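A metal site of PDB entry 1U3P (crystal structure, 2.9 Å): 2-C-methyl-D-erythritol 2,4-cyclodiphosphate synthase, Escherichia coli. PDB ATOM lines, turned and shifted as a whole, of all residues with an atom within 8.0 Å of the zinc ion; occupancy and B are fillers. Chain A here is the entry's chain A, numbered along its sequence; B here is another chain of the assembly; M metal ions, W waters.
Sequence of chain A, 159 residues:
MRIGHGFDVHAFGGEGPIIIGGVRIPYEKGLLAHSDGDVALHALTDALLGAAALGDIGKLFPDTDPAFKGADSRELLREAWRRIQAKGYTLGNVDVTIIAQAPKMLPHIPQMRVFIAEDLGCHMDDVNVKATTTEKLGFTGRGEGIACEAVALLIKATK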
ATOM      1  N   PHE A   7       5.786  -8.158 -19.230  1.00  0.00           N
ATOM      2  CA  PHE A   7       7.128  -7.829 -18.772  1.00  0.00           C
ATOM      3  C   PHE A   7       7.356  -8.483 -17.420  1.00  0.00           C
ATOM      4  O   PHE A   7       6.447  -8.490 -16.584  1.00  0.00           O
ATOM      5  CB  PHE A   7       7.260  -6.323 -18.648  1.00  0.00           C
ATOM      6  CG  PHE A   7       8.546  -5.894 -18.024  1.00  0.00           C
ATOM      7  CD1 PHE A   7       9.671  -5.735 -18.803  1.00  0.00           C
ATOM      8  CD2 PHE A   7       8.631  -5.686 -16.654  1.00  0.00           C
ATOM      9  CE1 PHE A   7      10.880  -5.373 -18.232  1.00  0.00           C
ATOM     10  CE2 PHE A   7       9.834  -5.330 -16.068  1.00  0.00           C
ATOM     11  CZ  PHE A   7      10.969  -5.173 -16.856  1.00  0.00           C
ATOM     12  N   ASP A   8       8.556  -9.005 -17.192  1.00  0.00           N
ATOM     13  CA  ASP A   8       8.873  -9.668 -15.941  1.00  0.00           C
ATOM     14  C   ASP A   8      10.368  -9.677 -15.624  1.00  0.00           C
ATOM     15  O   ASP A   8      11.207  -9.669 -16.524  1.00  0.00           O
ATOM     16  CB  ASP A   8       8.334 -11.083 -15.959  1.00  0.00           C
ATOM     17  CG  ASP A   8       8.313 -11.718 -14.593  1.00  0.00           C
ATOM     18  OD1 ASP A   8       8.368 -12.974 -14.536  1.00  0.00           O
ATOM     19  OD2 ASP A   8       8.246 -10.999 -13.578  1.00  0.00           O
ATOM     20  N   VAL A   9      10.691  -9.706 -14.325  1.00  0.00           N
ATOM     21  CA  VAL A   9      12.061  -9.698 -13.832  1.00  0.00           C
ATOM     22  C   VAL A   9      12.180 -10.629 -12.616  1.00  0.00           C
ATOM     23  O   VAL A   9      11.208 -10.814 -11.888  1.00  0.00           O
ATOM     24  CB  VAL A   9      12.443  -8.281 -13.350  1.00  0.00           C
ATOM     25  CG1 VAL A   9      13.773  -8.271 -12.631  1.00  0.00           C
ATOM     26  CG2 VAL A   9      12.518  -7.358 -14.524  1.00  0.00           C
ATOM     27  N   HIS A  10      13.320 -11.279 -12.457  1.00  0.00           N
ATOM     28  CA  HIS A  10      13.574 -12.162 -11.310  1.00  0.00           C
ATOM     29  C   HIS A  10      15.043 -12.035 -10.933  1.00  0.00           C
ATOM     30  O   HIS A  10      15.911 -11.875 -11.799  1.00  0.00           O
ATOM     31  CB  HIS A  10      13.224 -13.616 -11.599  1.00  0.00           C
ATOM     32  CG  HIS A  10      11.760 -13.890 -11.560  1.00  0.00           C
ATOM     33  ND1 HIS A  10      11.046 -13.952 -10.387  1.00  0.00           N
ATOM     34  CD2 HIS A  10      10.861 -14.075 -12.557  1.00  0.00           C
ATOM     35  CE1 HIS A  10       9.768 -14.165 -10.655  1.00  0.00           C
ATOM     36  NE2 HIS A  10       9.622 -14.237 -11.972  1.00  0.00           N
ATOM     37  N   LEU A  32      15.477 -16.451  -8.051  1.00  0.00           N
ATOM     38  CA  LEU A  32      14.562 -16.411  -6.927  1.00  0.00           C
ATOM     39  C   LEU A  32      13.115 -16.159  -7.345  1.00  0.00           C
ATOM     40  O   LEU A  32      12.831 -15.197  -8.057  1.00  0.00           O
ATOM     41  CB  LEU A  32      15.000 -15.326  -5.974  1.00  0.00           C
ATOM     42  CG  LEU A  32      16.440 -15.518  -5.550  1.00  0.00           C
ATOM     43  CD1 LEU A  32      16.819 -14.431  -4.599  1.00  0.00           C
ATOM     44  CD2 LEU A  32      16.580 -16.877  -4.894  1.00  0.00           C
ATOM     45  N   ALA A  33      12.210 -17.015  -6.874  1.00  0.00           N
ATOM     46  CA  ALA A  33      10.788 -16.860  -7.182  1.00  0.00           C
ATOM     47  C   ALA A  33       9.888 -17.845  -6.431  1.00  0.00           C
ATOM     48  O   ALA A  33      10.371 -18.847  -5.876  1.00  0.00           O
ATOM     49  CB  ALA A  33      10.574 -16.973  -8.669  1.00  0.00           C
ATOM     50  N   HIS A  34       8.583 -17.525  -6.375  1.00  0.00           N
ATOM     51  CA  HIS A  34       7.557 -18.370  -5.723  1.00  0.00           C
ATOM     52  C   HIS A  34       7.304 -19.590  -6.619  1.00  0.00           C
ATOM     53  O   HIS A  34       7.094 -20.681  -6.096  1.00  0.00           O
ATOM     54  CB  HIS A  34       6.265 -17.534  -5.484  1.00  0.00           C
ATOM     55  CG  HIS A  34       5.100 -18.292  -4.896  1.00  0.00           C
ATOM     56  ND1 HIS A  34       5.095 -18.786  -3.603  1.00  0.00           N
ATOM     57  CD2 HIS A  34       3.851 -18.528  -5.390  1.00  0.00           C
ATOM     58  CE1 HIS A  34       3.897 -19.286  -3.329  1.00  0.00           C
ATOM     59  NE2 HIS A  34       3.132 -19.142  -4.397  1.00  0.00           N
ATOM     60  N   SER A  35       7.276 -19.388  -7.934  1.00  0.00           N
ATOM     61  CA  SER A  35       7.084 -20.468  -8.905  1.00  0.00           C
ATOM     62  C   SER A  35       8.501 -20.878  -9.298  1.00  0.00           C
ATOM     63  O   SER A  35       9.425 -20.705  -8.511  1.00  0.00           O
ATOM     64  CB  SER A  35       6.368 -19.933 -10.141  1.00  0.00           C
ATOM     65  OG  SER A  35       7.242 -19.090 -10.883  1.00  0.00           O
ATOM     66  N   ASP A  36       8.684 -21.366 -10.518  1.00  0.00           N
ATOM     67  CA  ASP A  36      10.016 -21.743 -10.963  1.00  0.00           C
ATOM     68  C   ASP A  36      10.784 -20.499 -11.439  1.00  0.00           C
ATOM     69  O   ASP A  36      11.907 -20.591 -11.953  1.00  0.00           O
ATOM     70  CB  ASP A  36       9.916 -22.766 -12.081  1.00  0.00           C
ATOM     71  CG  ASP A  36       9.098 -22.266 -13.225  1.00  0.00           C
ATOM     72  OD1 ASP A  36       8.818 -23.055 -14.146  1.00  0.00           O
ATOM     73  OD2 ASP A  36       8.711 -21.088 -13.192  1.00  0.00           O
ATOM     74  N   GLY A  37      10.135 -19.348 -11.349  1.00  0.00           N
ATOM     75  CA  GLY A  37      10.785 -18.113 -11.741  1.00  0.00           C
ATOM     76  C   GLY A  37      11.165 -17.971 -13.196  1.00  0.00           C
ATOM     77  O   GLY A  37      12.037 -17.176 -13.520  1.00  0.00           O
ATOM     78  N   ASP A  38      10.469 -18.694 -14.070  1.00  0.00           N
ATOM     79  CA  ASP A  38      10.720 -18.627 -15.509  1.00  0.00           C
ATOM     80  C   ASP A  38      10.283 -17.258 -16.068  1.00  0.00           C
ATOM     81  O   ASP A  38       9.143 -17.098 -16.512  1.00  0.00           O
ATOM     82  CB  ASP A  38       9.942 -19.737 -16.198  1.00  0.00           C
ATOM     83  CG  ASP A  38      10.294 -19.912 -17.657  1.00  0.00           C
ATOM     84  OD1 ASP A  38      10.629 -18.921 -18.346  1.00  0.00           O
ATOM     85  OD2 ASP A  38      10.211 -21.048 -18.134  1.00  0.00           O
ATOM     86  N   VAL A  39      11.177 -16.266 -16.018  1.00  0.00           N
ATOM     87  CA  VAL A  39      10.871 -14.925 -16.507  1.00  0.00           C
ATOM     88  C   VAL A  39      10.267 -14.914 -17.896  1.00  0.00           C
ATOM     89  O   VAL A  39       9.277 -14.248 -18.124  1.00  0.00           O
ATOM     90  CB  VAL A  39      12.113 -14.044 -16.572  1.00  0.00           C
ATOM     91  CG1 VAL A  39      11.718 -12.619 -16.678  1.00  0.00           C
ATOM     92  CG2 VAL A  39      12.916 -14.206 -15.347  1.00  0.00           C
ATOM     93  N   ALA A  40      10.827 -15.687 -18.816  1.00  0.00           N
ATOM     94  CA  ALA A  40      10.339 -15.718 -20.191  1.00  0.00           C
ATOM     95  C   ALA A  40       8.875 -16.044 -20.302  1.00  0.00           C
ATOM     96  O   ALA A  40       8.121 -15.347 -20.966  1.00  0.00           O
ATOM     97  CB  ALA A  40      11.133 -16.728 -21.022  1.00  0.00           C
ATOM     98  N   LEU A  41       8.462 -17.115 -19.646  1.00  0.00           N
ATOM     99  CA  LEU A  41       7.076 -17.500 -19.749  1.00  0.00           C
ATOM    100  C   LEU A  41       6.108 -16.613 -18.976  1.00  0.00           C
ATOM    101  O   LEU A  41       4.952 -16.475 -19.382  1.00  0.00           O
ATOM    102  CB  LEU A  41       6.909 -18.969 -19.397  1.00  0.00           C
ATOM    103  CG  LEU A  41       7.724 -19.923 -20.264  1.00  0.00           C
ATOM    104  CD1 LEU A  41       7.386 -21.344 -19.891  1.00  0.00           C
ATOM    105  CD2 LEU A  41       7.433 -19.687 -21.729  1.00  0.00           C
ATOM    106  N   HIS A  42       6.555 -15.997 -17.888  1.00  0.00           N
ATOM    107  CA  HIS A  42       5.642 -15.104 -17.170  1.00  0.00           C
ATOM    108  C   HIS A  42       5.322 -13.947 -18.077  1.00  0.00           C
ATOM    109  O   HIS A  42       4.171 -13.605 -18.243  1.00  0.00           O
ATOM    110  CB  HIS A  42       6.240 -14.577 -15.890  1.00  0.00           C
ATOM    111  CG  HIS A  42       6.483 -15.640 -14.879  1.00  0.00           C
ATOM    112  ND1 HIS A  42       7.222 -15.426 -13.734  1.00  0.00           N
ATOM    113  CD2 HIS A  42       6.112 -16.941 -14.845  1.00  0.00           C
ATOM    114  CE1 HIS A  42       7.300 -16.549 -13.047  1.00  0.00           C
ATOM    115  NE2 HIS A  42       6.631 -17.484 -13.703  1.00  0.00           N
ATOM    116  N   ALA A  43       6.342 -13.387 -18.713  1.00  0.00           N
ATOM    117  CA  ALA A  43       6.107 -12.279 -19.607  1.00  0.00           C
ATOM    118  C   ALA A  43       5.183 -12.705 -20.748  1.00  0.00           C
ATOM    119  O   ALA A  43       4.220 -12.015 -21.074  1.00  0.00           O
ATOM    120  CB  ALA A  43       7.388 -11.740 -20.129  1.00  0.00           C
ATOM    121  N   ASP A  46       1.534 -12.967 -19.411  1.00  0.00           N
ATOM    122  CA  ASP A  46       0.869 -11.683 -19.271  1.00  0.00           C
ATOM    123  C   ASP A  46       0.510 -11.051 -20.595  1.00  0.00           C
ATOM    124  O   ASP A  46      -0.469 -10.311 -20.674  1.00  0.00           O
ATOM    125  CB  ASP A  46       1.746 -10.700 -18.534  1.00  0.00           C
ATOM    126  CG  ASP A  46       1.686 -10.879 -17.066  1.00  0.00           C
ATOM    127  OD1 ASP A  46       2.443 -10.181 -16.361  1.00  0.00           O
ATOM    128  OD2 ASP A  46       0.892 -11.720 -16.633  1.00  0.00           O
ATOM    129  N   ILE A  57      -0.929 -12.496 -14.743  1.00  0.00           N
ATOM    130  CA  ILE A  57      -0.618 -13.741 -14.074  1.00  0.00           C
ATOM    131  C   ILE A  57      -0.658 -13.591 -12.549  1.00  0.00           C
ATOM    132  O   ILE A  57      -1.072 -14.518 -11.859  1.00  0.00           O
ATOM    133  CB  ILE A  57       0.736 -14.317 -14.597  1.00  0.00           C
ATOM    134  CG1 ILE A  57       0.714 -15.830 -14.520  1.00  0.00           C
ATOM    135  CG2 ILE A  57       1.935 -13.781 -13.829  1.00  0.00           C
ATOM    136  CD1 ILE A  57       2.020 -16.461 -14.964  1.00  0.00           C
ATOM    137  N   ASP A  63       1.055 -14.853  -5.480  1.00  0.00           N
ATOM    138  CA  ASP A  63       2.241 -15.240  -4.693  1.00  0.00           C
ATOM    139  C   ASP A  63       1.734 -15.782  -3.401  1.00  0.00           C
ATOM    140  O   ASP A  63       2.338 -16.670  -2.791  1.00  0.00           O
ATOM    141  CB  ASP A  63       3.084 -14.020  -4.330  1.00  0.00           C
ATOM    142  CG  ASP A  63       3.694 -13.357  -5.528  1.00  0.00           C
ATOM    143  OD1 ASP A  63       2.945 -13.098  -6.488  1.00  0.00           O
ATOM    144  OD2 ASP A  63       4.912 -13.095  -5.505  1.00  0.00           O
ATOM    145  N   SER A  73       5.981 -22.942 -14.670  1.00  0.00           N
ATOM    146  CA  SER A  73       5.367 -21.876 -15.445  1.00  0.00           C
ATOM    147  C   SER A  73       4.656 -22.280 -16.734  1.00  0.00           C
ATOM    148  O   SER A  73       3.814 -21.531 -17.228  1.00  0.00           O
ATOM    149  CB  SER A  73       6.357 -20.767 -15.720  1.00  0.00           C
ATOM    150  OG  SER A  73       6.687 -20.121 -14.501  1.00  0.00           O
ATOM    151  N   ILE A 146      17.362 -11.273 -14.331  1.00  0.00           N
ATOM    152  CA  ILE A 146      17.035 -11.407 -15.751  1.00  0.00           C
ATOM    153  C   ILE A 146      15.658 -10.825 -15.956  1.00  0.00           C
ATOM    154  O   ILE A 146      14.759 -11.054 -15.146  1.00  0.00           O
ATOM    155  CB  ILE A 146      16.994 -12.900 -16.213  1.00  0.00           C
ATOM    156  CG1 ILE A 146      18.403 -13.466 -16.348  1.00  0.00           C
ATOM    157  CG2 ILE A 146      16.300 -13.029 -17.557  1.00  0.00           C
ATOM    158  CD1 ILE A 146      18.434 -14.905 -16.823  1.00  0.00           C
ATOM    159  N   THR B 132       3.466  -5.224 -12.311  1.00  0.00           N
ATOM    160  CA  THR B 132       4.588  -6.094 -12.013  1.00  0.00           C
ATOM    161  C   THR B 132       5.673  -5.392 -11.199  1.00  0.00           C
ATOM    162  O   THR B 132       5.810  -4.172 -11.244  1.00  0.00           O
ATOM    163  CB  THR B 132       5.215  -6.627 -13.314  1.00  0.00           C
ATOM    164  OG1 THR B 132       6.222  -7.592 -12.983  1.00  0.00           O
ATOM    165  CG2 THR B 132       5.857  -5.501 -14.127  1.00  0.00           C
ATOM    166  N   THR B 133       6.478  -6.202 -10.519  1.00  0.00           N
ATOM    167  CA  THR B 133       7.590  -5.739  -9.680  1.00  0.00           C
ATOM    168  C   THR B 133       8.895  -6.138 -10.338  1.00  0.00           C
ATOM    169  O   THR B 133       8.934  -7.073 -11.131  1.00  0.00           O
ATOM    170  CB  THR B 133       7.569  -6.495  -8.353  1.00  0.00           C
ATOM    171  OG1 THR B 133       6.383  -6.169  -7.632  1.00  0.00           O
ATOM    172  CG2 THR B 133       8.732  -6.150  -7.518  1.00  0.00           C
ATOM    173  N   GLU B 135      11.293  -7.170  -8.551  1.00  0.00           N
ATOM    174  CA  GLU B 135      11.790  -7.954  -7.415  1.00  0.00           C
ATOM    175  C   GLU B 135      12.971  -7.291  -6.691  1.00  0.00           C
ATOM    176  O   GLU B 135      14.005  -7.911  -6.463  1.00  0.00           O
ATOM    177  CB  GLU B 135      12.146  -9.385  -7.846  1.00  0.00           C
ATOM    178  CG  GLU B 135      11.069 -10.136  -8.636  1.00  0.00           C
ATOM    179  CD  GLU B 135       9.848 -10.551  -7.805  1.00  0.00           C
ATOM    180  OE1 GLU B 135       9.158  -9.661  -7.254  1.00  0.00           O
ATOM    181  OE2 GLU B 135       9.572 -11.763  -7.743  1.00  0.00           O
HETATM  182 ZN    ZN M   1       7.922 -13.817 -12.844  1.00  0.00          ZN
HETATM  183  O   HOH W   1       6.676 -13.390 -11.412  1.00  0.00           O
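Within 4 Å of the zinc ion: Asp 8, His 10 and His 42.
The zinc ion is bound by OD1 of Asp 8, 1.9 Å away.
Water W1 is bound to the zinc ion (1.9 Å).
NE2 of His 10 is bound to the zinc ion, 2.0 Å away.
The zinc ion is bound by a ring nitrogen (ND1) of His 42.
The zinc ion has four donor atoms within binding distance.
The backbone NH (N) of Ile 146 is in hydrogen-bond range of the backbone carbonyl oxygen (O) of His 10 (3.0 Å).
OG of Ser 73 is in hydrogen-bond range of NE2 of His 42, 2.8 Å away.
ND1 of His 10 lies within hydrogen-bond range of O of Leu 32 (3.2 Å).
OG of Ser 35 sits at hydrogen-bond distance from NE2 of His 42 (3.3 Å).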
